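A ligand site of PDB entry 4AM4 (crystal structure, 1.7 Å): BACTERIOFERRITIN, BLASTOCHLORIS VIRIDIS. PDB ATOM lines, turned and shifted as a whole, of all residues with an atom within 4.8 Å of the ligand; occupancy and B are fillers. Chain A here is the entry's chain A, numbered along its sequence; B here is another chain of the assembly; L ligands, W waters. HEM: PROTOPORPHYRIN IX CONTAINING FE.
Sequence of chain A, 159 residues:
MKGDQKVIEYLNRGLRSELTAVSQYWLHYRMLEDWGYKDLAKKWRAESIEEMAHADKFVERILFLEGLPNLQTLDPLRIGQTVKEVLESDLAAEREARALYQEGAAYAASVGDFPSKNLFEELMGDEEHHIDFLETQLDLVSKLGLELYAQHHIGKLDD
The side-chain sulfur of Met 52 of chain A is bound to an iron atom (FE) of the ligand (2.3 Å). An iron atom (FE) of the ligand is bound by the side-chain sulfur (SD) of Met 52 of chain B, at 2.3 Å. The guanidinium group (NH1) of Arg 45 of chain B is in salt-bridge range of an oxygen (O1A) of the ligand (3.1 Å). The guanidinium group of Arg 45 of chain A is in salt-bridge range of an oxygen (O2D) of the ligand, 3.0 Å away.
The side-chain carboxylate of Asp 56 of chain B sits at hydrogen-bond distance from the indole nitrogen of Trp 26 of chain A, 2.8 Å away. The indole nitrogen (NE1) of Trp 26 of chain B sits at hydrogen-bond distance from the side-chain carboxylate (OD1) of Asp 56 of chain A.
CD2 of Leu 19 of chain A touches CAB of the ligand, at 3.6 Å. Val 22 of chain A touches the ligand. Trp 26 of chain A touches the ligand. CD1 of Ile 49 of chain A touches CBD of the ligand, at 3.7 Å. Leu 19 of chain B touches the ligand (CD2 to CMC, 3.6 Å). CG1 of Val 22 of chain B touches CHC of the ligand, at 3.7 Å. Ser 23 of chain B touches the ligand. Trp 26 of chain B touches the ligand. Ile 49 of chain B touches the ligand (CD1 to CBA, 3.7 Å). Ala 55 of chain B touches the ligand. Hydrophobic or aromatic side chains that line the ligand: Leu 19 of chain A, Val 22 of chain A, Trp 26 of chain A, Ile 49 of chain A, Met 52 of chain A, Leu 19 of chain B, Val 22 of chain B, Trp 26 of chain B, Ile 49 of chain B, Met 52 of chain B and Ala 55 of chain B. Within 4 Å of the ligand: Leu 19 of chain A, Val 22 of chain A, Trp 26 of chain A, Arg 45 of chain A, Ile 49 of chain A, Met 52 of chain A, Leu 19 of chain B, Val 22 of chain B, Ser 23 of chain B, Trp 26 of chain B, Arg 45 of chain B, Ile 49 of chain B, Met 52 of chain B and Ala 55 of chain B. The nearest printed residue that does not touch the ligand is Ser 23 of chain A (4.05 Å).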
ATOM      1  N   LEU A  19     -28.872  14.779 -22.013  1.00  0.00           N
ATOM      2  CA  LEU A  19     -28.995  16.234 -22.165  1.00  0.00           C
ATOM      3  C   LEU A  19     -28.593  16.970 -20.842  1.00  0.00           C
ATOM      4  O   LEU A  19     -28.010  18.094 -20.852  1.00  0.00           O
ATOM      5  CB  LEU A  19     -30.436  16.664 -22.551  1.00  0.00           C
ATOM      6  CG  LEU A  19     -30.920  16.175 -23.930  1.00  0.00           C
ATOM      7  CD1 LEU A  19     -32.410  16.395 -24.017  1.00  0.00           C
ATOM      8  CD2 LEU A  19     -30.148  16.991 -24.989  1.00  0.00           C
ATOM      9  N   VAL A  22     -24.783  16.899 -20.763  1.00  0.00           N
ATOM     10  CA  VAL A  22     -24.185  17.890 -21.710  1.00  0.00           C
ATOM     11  C   VAL A  22     -24.142  19.263 -21.023  1.00  0.00           C
ATOM     12  O   VAL A  22     -23.106  19.945 -21.054  1.00  0.00           O
ATOM     13  CB  VAL A  22     -25.051  18.051 -22.990  1.00  0.00           C
ATOM     14  CG1 VAL A  22     -24.570  19.289 -23.794  1.00  0.00           C
ATOM     15  CG2 VAL A  22     -24.880  16.757 -23.850  1.00  0.00           C
ATOM     16  N   SER A  23     -25.266  19.739 -20.483  1.00  0.00           N
ATOM     17  CA  SER A  23     -25.289  21.092 -19.913  1.00  0.00           C
ATOM     18  C   SER A  23     -24.517  21.199 -18.592  1.00  0.00           C
ATOM     19  O   SER A  23     -23.880  22.249 -18.324  1.00  0.00           O
ATOM     20  CB  SER A  23     -26.740  21.556 -19.655  1.00  0.00           C
ATOM     21  OG  SER A  23     -27.347  21.846 -20.905  1.00  0.00           O
ATOM     22  N   TRP A  26     -20.923  21.214 -19.602  1.00  0.00           N
ATOM     23  CA  TRP A  26     -20.521  22.471 -20.337  1.00  0.00           C
ATOM     24  C   TRP A  26     -20.418  23.583 -19.342  1.00  0.00           C
ATOM     25  O   TRP A  26     -19.506  24.410 -19.342  1.00  0.00           O
ATOM     26  CB  TRP A  26     -21.617  22.840 -21.382  1.00  0.00           C
ATOM     27  CG  TRP A  26     -21.020  23.873 -22.313  1.00  0.00           C
ATOM     28  CD1 TRP A  26     -21.078  25.243 -22.196  1.00  0.00           C
ATOM     29  CD2 TRP A  26     -20.117  23.597 -23.418  1.00  0.00           C
ATOM     30  NE1 TRP A  26     -20.265  25.864 -23.180  1.00  0.00           N
ATOM     31  CE2 TRP A  26     -19.681  24.904 -23.941  1.00  0.00           C
ATOM     32  CE3 TRP A  26     -19.693  22.433 -24.038  1.00  0.00           C
ATOM     33  CZ2 TRP A  26     -18.815  25.020 -25.050  1.00  0.00           C
ATOM     34  CZ3 TRP A  26     -18.820  22.521 -25.123  1.00  0.00           C
ATOM     35  CH2 TRP A  26     -18.397  23.759 -25.630  1.00  0.00           C
ATOM     36  N   ARG A  45     -14.763  20.309 -21.424  1.00  0.00           N
ATOM     37  CA  ARG A  45     -15.337  20.659 -22.777  1.00  0.00           C
ATOM     38  C   ARG A  45     -15.431  19.372 -23.611  1.00  0.00           C
ATOM     39  O   ARG A  45     -16.432  19.117 -24.237  1.00  0.00           O
ATOM     40  CB  ARG A  45     -14.430  21.692 -23.446  1.00  0.00           C
ATOM     41  CG  ARG A  45     -15.090  22.297 -24.664  1.00  0.00           C
ATOM     42  CD  ARG A  45     -14.149  23.355 -25.281  1.00  0.00           C
ATOM     43  NE  ARG A  45     -14.890  24.197 -26.248  1.00  0.00           N
ATOM     44  CZ  ARG A  45     -15.003  23.933 -27.522  1.00  0.00           C
ATOM     45  NH1 ARG A  45     -14.523  22.787 -27.944  1.00  0.00           N
ATOM     46  NH2 ARG A  45     -15.629  24.787 -28.355  1.00  0.00           N
ATOM     47  N   ILE A  49     -18.850  17.352 -25.050  1.00  0.00           N
ATOM     48  CA  ILE A  49     -19.022  17.032 -26.498  1.00  0.00           C
ATOM     49  C   ILE A  49     -19.191  15.510 -26.669  1.00  0.00           C
ATOM     50  O   ILE A  49     -19.991  15.108 -27.539  1.00  0.00           O
ATOM     51  CB  ILE A  49     -17.850  17.655 -27.295  1.00  0.00           C
ATOM     52  CG1 ILE A  49     -18.161  19.136 -27.321  1.00  0.00           C
ATOM     53  CG2 ILE A  49     -18.003  17.163 -28.743  1.00  0.00           C
ATOM     54  CD1 ILE A  49     -16.904  19.918 -27.820  1.00  0.00           C
ATOM     55  N   MET A  52     -22.751  14.952 -25.954  1.00  0.00           N
ATOM     56  CA  MET A  52     -23.577  15.411 -27.056  1.00  0.00           C
ATOM     57  C   MET A  52     -23.708  14.268 -28.071  1.00  0.00           C
ATOM     58  O   MET A  52     -24.811  14.024 -28.610  1.00  0.00           O
ATOM     59  CB  MET A  52     -22.933  16.641 -27.717  1.00  0.00           C
ATOM     60  CG  MET A  52     -22.998  17.844 -26.743  1.00  0.00           C
ATOM     61  SD  MET A  52     -22.050  19.182 -27.570  1.00  0.00           S
ATOM     62  CE  MET A  52     -21.540  20.107 -26.050  1.00  0.00           C
ATOM     63  N   ALA A  53     -22.662  13.510 -28.330  1.00  0.00           N
ATOM     64  CA  ALA A  53     -22.781  12.414 -29.277  1.00  0.00           C
ATOM     65  C   ALA A  53     -23.732  11.298 -28.746  1.00  0.00           C
ATOM     66  O   ALA A  53     -24.456  10.683 -29.504  1.00  0.00           O
ATOM     67  CB  ALA A  53     -21.389  11.808 -29.558  1.00  0.00           C
ATOM     68  N   ALA A  55     -26.236  11.808 -26.680  1.00  0.00           N
ATOM     69  CA  ALA A  55     -27.623  12.381 -26.841  1.00  0.00           C
ATOM     70  C   ALA A  55     -28.110  12.118 -28.273  1.00  0.00           C
ATOM     71  O   ALA A  55     -29.236  11.655 -28.479  1.00  0.00           O
ATOM     72  CB  ALA A  55     -27.671  13.875 -26.471  1.00  0.00           C
ATOM     73  N   ASP A  56     -27.230  12.427 -29.247  1.00  0.00           N
ATOM     74  CA  ASP A  56     -27.643  12.240 -30.617  1.00  0.00           C
ATOM     75  C   ASP A  56     -27.914  10.776 -30.939  1.00  0.00           C
ATOM     76  O   ASP A  56     -28.834  10.471 -31.651  1.00  0.00           O
ATOM     77  CB  ASP A  56     -26.450  12.743 -31.511  1.00  0.00           C
ATOM     78  CG  ASP A  56     -26.812  12.656 -32.966  1.00  0.00           C
ATOM     79  OD1 ASP A  56     -27.921  13.013 -33.424  1.00  0.00           O
ATOM     80  OD2 ASP A  56     -25.982  12.193 -33.737  1.00  0.00           O
ATOM     81  N   LEU A  71     -36.817  16.379 -26.005  1.00  0.00           N
ATOM     82  CA  LEU A  71     -35.649  17.176 -25.554  1.00  0.00           C
ATOM     83  C   LEU A  71     -36.125  18.306 -24.685  1.00  0.00           C
ATOM     84  O   LEU A  71     -35.331  19.186 -24.380  1.00  0.00           O
ATOM     85  CB  LEU A  71     -34.893  17.722 -26.811  1.00  0.00           C
ATOM     86  CG  LEU A  71     -34.207  16.577 -27.592  1.00  0.00           C
ATOM     87  CD1 LEU A  71     -35.137  15.888 -28.642  1.00  0.00           C
ATOM     88  CD2 LEU A  71     -33.077  17.274 -28.372  1.00  0.00           C
ATOM     89  N   LEU B  19     -30.620  27.657 -25.872  1.00  0.00           N
ATOM     90  CA  LEU B  19     -30.695  26.240 -25.576  1.00  0.00           C
ATOM     91  C   LEU B  19     -31.915  25.592 -26.251  1.00  0.00           C
ATOM     92  O   LEU B  19     -31.915  24.423 -26.700  1.00  0.00           O
ATOM     93  CB  LEU B  19     -30.769  25.920 -24.044  1.00  0.00           C
ATOM     94  CG  LEU B  19     -29.491  26.404 -23.285  1.00  0.00           C
ATOM     95  CD1 LEU B  19     -29.699  26.384 -21.789  1.00  0.00           C
ATOM     96  CD2 LEU B  19     -28.320  25.451 -23.660  1.00  0.00           C
ATOM     97  N   VAL B  22     -31.075  25.227 -29.897  1.00  0.00           N
ATOM     98  CA  VAL B  22     -30.167  24.106 -30.197  1.00  0.00           C
ATOM     99  C   VAL B  22     -30.950  22.795 -30.284  1.00  0.00           C
ATOM    100  O   VAL B  22     -30.757  22.006 -31.213  1.00  0.00           O
ATOM    101  CB  VAL B  22     -29.156  23.921 -29.029  1.00  0.00           C
ATOM    102  CG1 VAL B  22     -28.381  22.588 -29.162  1.00  0.00           C
ATOM    103  CG2 VAL B  22     -28.123  25.070 -29.015  1.00  0.00           C
ATOM    104  N   SER B  23     -31.784  22.508 -29.275  1.00  0.00           N
ATOM    105  CA  SER B  23     -32.507  21.265 -29.271  1.00  0.00           C
ATOM    106  C   SER B  23     -33.617  21.153 -30.310  1.00  0.00           C
ATOM    107  O   SER B  23     -33.829  20.081 -30.917  1.00  0.00           O
ATOM    108  CB  SER B  23     -33.137  20.991 -27.884  1.00  0.00           C
ATOM    109  OG  SER B  23     -32.109  20.626 -27.019  1.00  0.00           O
ATOM    110  N   TRP B  26     -31.747  20.622 -33.506  1.00  0.00           N
ATOM    111  CA  TRP B  26     -31.077  19.284 -33.602  1.00  0.00           C
ATOM    112  C   TRP B  26     -32.149  18.242 -33.863  1.00  0.00           C
ATOM    113  O   TRP B  26     -32.012  17.306 -34.673  1.00  0.00           O
ATOM    114  CB  TRP B  26     -30.371  18.951 -32.264  1.00  0.00           C
ATOM    115  CG  TRP B  26     -29.463  17.767 -32.487  1.00  0.00           C
ATOM    116  CD1 TRP B  26     -29.771  16.410 -32.338  1.00  0.00           C
ATOM    117  CD2 TRP B  26     -28.145  17.812 -33.106  1.00  0.00           C
ATOM    118  NE1 TRP B  26     -28.691  15.612 -32.790  1.00  0.00           N
ATOM    119  CE2 TRP B  26     -27.690  16.442 -33.255  1.00  0.00           C
ATOM    120  CE3 TRP B  26     -27.305  18.865 -33.482  1.00  0.00           C
ATOM    121  CZ2 TRP B  26     -26.421  16.132 -33.825  1.00  0.00           C
ATOM    122  CZ3 TRP B  26     -26.077  18.607 -34.042  1.00  0.00           C
ATOM    123  CH2 TRP B  26     -25.606  17.280 -34.163  1.00  0.00           C
ATOM    124  N   ARG B  45     -28.385  20.624 -39.082  1.00  0.00           N
ATOM    125  CA  ARG B  45     -27.284  20.233 -38.155  1.00  0.00           C
ATOM    126  C   ARG B  45     -26.350  21.437 -37.998  1.00  0.00           C
ATOM    127  O   ARG B  45     -25.936  21.773 -36.866  1.00  0.00           O
ATOM    128  CB  ARG B  45     -26.542  19.005 -38.749  1.00  0.00           C
ATOM    129  CG  ARG B  45     -25.648  18.347 -37.710  1.00  0.00           C
ATOM    130  CD  ARG B  45     -24.878  17.184 -38.357  1.00  0.00           C
ATOM    131  NE  ARG B  45     -24.245  16.308 -37.338  1.00  0.00           N
ATOM    132  CZ  ARG B  45     -23.012  16.474 -36.958  1.00  0.00           C
ATOM    133  NH1 ARG B  45     -22.383  17.532 -37.421  1.00  0.00           N
ATOM    134  NH2 ARG B  45     -22.439  15.614 -36.100  1.00  0.00           N
ATOM    135  N   ILE B  49     -25.558  23.679 -34.489  1.00  0.00           N
ATOM    136  CA  ILE B  49     -24.166  23.942 -34.007  1.00  0.00           C
ATOM    137  C   ILE B  49     -23.845  25.442 -33.926  1.00  0.00           C
ATOM    138  O   ILE B  49     -23.158  25.846 -32.959  1.00  0.00           O
ATOM    139  CB  ILE B  49     -23.186  23.116 -34.865  1.00  0.00           C
ATOM    140  CG1 ILE B  49     -23.434  21.641 -34.483  1.00  0.00           C
ATOM    141  CG2 ILE B  49     -21.785  23.481 -34.372  1.00  0.00           C
ATOM    142  CD1 ILE B  49     -22.715  20.659 -35.439  1.00  0.00           C
ATOM    143  N   MET B  52     -25.337  26.446 -30.750  1.00  0.00           N
ATOM    144  CA  MET B  52     -24.568  25.973 -29.593  1.00  0.00           C
ATOM    145  C   MET B  52     -23.459  27.057 -29.301  1.00  0.00           C
ATOM    146  O   MET B  52     -23.179  27.356 -28.151  1.00  0.00           O
ATOM    147  CB  MET B  52     -23.898  24.641 -29.932  1.00  0.00           C
ATOM    148  CG  MET B  52     -24.991  23.546 -30.029  1.00  0.00           C
ATOM    149  SD  MET B  52     -24.112  22.036 -30.597  1.00  0.00           S
ATOM    150  CE  MET B  52     -25.542  21.223 -31.363  1.00  0.00           C
ATOM    151  N   ALA B  55     -25.125  29.902 -27.467  1.00  0.00           N
ATOM    152  CA  ALA B  55     -25.376  29.493 -26.049  1.00  0.00           C
ATOM    153  C   ALA B  55     -24.097  29.682 -25.230  1.00  0.00           C
ATOM    154  O   ALA B  55     -24.119  30.291 -24.149  1.00  0.00           O
ATOM    155  CB  ALA B  55     -25.913  28.057 -25.931  1.00  0.00           C
ATOM    156  N   ASP B  56     -22.981  29.163 -25.797  1.00  0.00           N
ATOM    157  CA  ASP B  56     -21.742  29.273 -25.066  1.00  0.00           C
ATOM    158  C   ASP B  56     -21.310  30.716 -24.823  1.00  0.00           C
ATOM    159  O   ASP B  56     -20.807  31.043 -23.760  1.00  0.00           O
ATOM    160  CB  ASP B  56     -20.651  28.556 -25.920  1.00  0.00           C
ATOM    161  CG  ASP B  56     -19.311  28.543 -25.194  1.00  0.00           C
ATOM    162  OD1 ASP B  56     -19.182  28.287 -23.988  1.00  0.00           O
ATOM    163  OD2 ASP B  56     -18.300  28.842 -25.848  1.00  0.00           O
ATOM    164  N   LEU B  71     -28.900  26.675 -17.070  1.00  0.00           N
ATOM    165  CA  LEU B  71     -29.131  25.800 -18.236  1.00  0.00           C
ATOM    166  C   LEU B  71     -30.236  24.837 -17.912  1.00  0.00           C
ATOM    167  O   LEU B  71     -30.441  23.883 -18.652  1.00  0.00           O
ATOM    168  CB  LEU B  71     -27.796  25.031 -18.548  1.00  0.00           C
ATOM    169  CG  LEU B  71     -26.776  26.028 -19.159  1.00  0.00           C
ATOM    170  CD1 LEU B  71     -25.975  26.736 -18.047  1.00  0.00           C
ATOM    171  CD2 LEU B  71     -25.834  25.098 -19.960  1.00  0.00           C
HETATM  172  CHA HEM L   1     -20.605  20.428 -31.070  1.00  0.00           C
HETATM  173  CHB HEM L   1     -24.657  17.838 -30.464  1.00  0.00           C
HETATM  174  CHC HEM L   1     -25.985  20.878 -26.896  1.00  0.00           C
HETATM  175  CHD HEM L   1     -21.831  23.476 -27.510  1.00  0.00           C
HETATM  176  C1A HEM L   1     -21.548  19.392 -31.154  1.00  0.00           C
HETATM  177  C2A HEM L   1     -21.366  18.206 -31.933  1.00  0.00           C
HETATM  178  C3A HEM L   1     -22.548  17.449 -31.782  1.00  0.00           C
HETATM  179  C4A HEM L   1     -23.394  18.237 -30.873  1.00  0.00           C
HETATM  180  CMA HEM L   1     -22.926  16.079 -32.288  1.00  0.00           C
HETATM  181  CAA HEM L   1     -20.046  17.879 -32.667  1.00  0.00           C
HETATM  182  CBA HEM L   1     -20.441  18.139 -34.079  1.00  0.00           C
HETATM  183  CGA HEM L   1     -19.268  17.754 -35.008  1.00  0.00           C
HETATM  184  O1A HEM L   1     -19.555  17.605 -36.264  1.00  0.00           O
HETATM  185  O2A HEM L   1     -18.108  17.616 -34.464  1.00  0.00           O
HETATM  186  C1B HEM L   1     -25.402  18.523 -29.472  1.00  0.00           C
HETATM  187  C2B HEM L   1     -26.732  18.039 -29.022  1.00  0.00           C
HETATM  188  C3B HEM L   1     -27.050  18.974 -28.053  1.00  0.00           C
HETATM  189  C4B HEM L   1     -25.963  19.872 -27.916  1.00  0.00           C
HETATM  190  CMB HEM L   1     -27.553  16.881 -29.596  1.00  0.00           C
HETATM  191  CAB HEM L   1     -28.279  19.056 -27.253  1.00  0.00           C
HETATM  192  CBB HEM L   1     -29.268  18.826 -28.133  1.00  0.00           C
HETATM  193  C1C HEM L   1     -24.910  21.765 -26.669  1.00  0.00           C
HETATM  194  C2C HEM L   1     -24.916  22.765 -25.606  1.00  0.00           C
HETATM  195  C3C HEM L   1     -23.783  23.545 -25.847  1.00  0.00           C
HETATM  196  C4C HEM L   1     -23.023  22.919 -26.955  1.00  0.00           C
HETATM  197  CMC HEM L   1     -26.020  22.844 -24.598  1.00  0.00           C
HETATM  198  CAC HEM L   1     -23.161  24.647 -25.050  1.00  0.00           C
HETATM  199  CBC HEM L   1     -24.016  25.338 -24.315  1.00  0.00           C
HETATM  200  C1D HEM L   1     -21.193  22.834 -28.601  1.00  0.00           C
HETATM  201  C2D HEM L   1     -20.004  23.404 -29.219  1.00  0.00           C
HETATM  202  C3D HEM L   1     -19.648  22.512 -30.249  1.00  0.00           C
HETATM  203  C4D HEM L   1     -20.624  21.485 -30.146  1.00  0.00           C
HETATM  204  CMD HEM L   1     -19.368  24.694 -28.763  1.00  0.00           C
HETATM  205  CAD HEM L   1     -18.534  22.495 -31.333  1.00  0.00           C
HETATM  206  CBD HEM L   1     -17.264  22.380 -30.535  1.00  0.00           C
HETATM  207  CGD HEM L   1     -16.064  22.545 -31.495  1.00  0.00           C
HETATM  208  O1D HEM L   1     -16.336  22.695 -32.770  1.00  0.00           O
HETATM  209  O2D HEM L   1     -14.897  22.500 -30.919  1.00  0.00           O
HETATM  210  NA  HEM L   1     -22.726  19.403 -30.442  1.00  0.00           N
HETATM  211  NB  HEM L   1     -24.948  19.607 -28.786  1.00  0.00           N
HETATM  212  NC  HEM L   1     -23.755  21.842 -27.515  1.00  0.00           N
HETATM  213  ND  HEM L   1     -21.582  21.691 -29.253  1.00  0.00           N
HETATM  214 FE   HEM L   1     -23.246  20.624 -28.969  1.00  0.00          FE
HETATM  215  O   HOH W   1     -18.088  27.933 -28.697  1.00  0.00           O
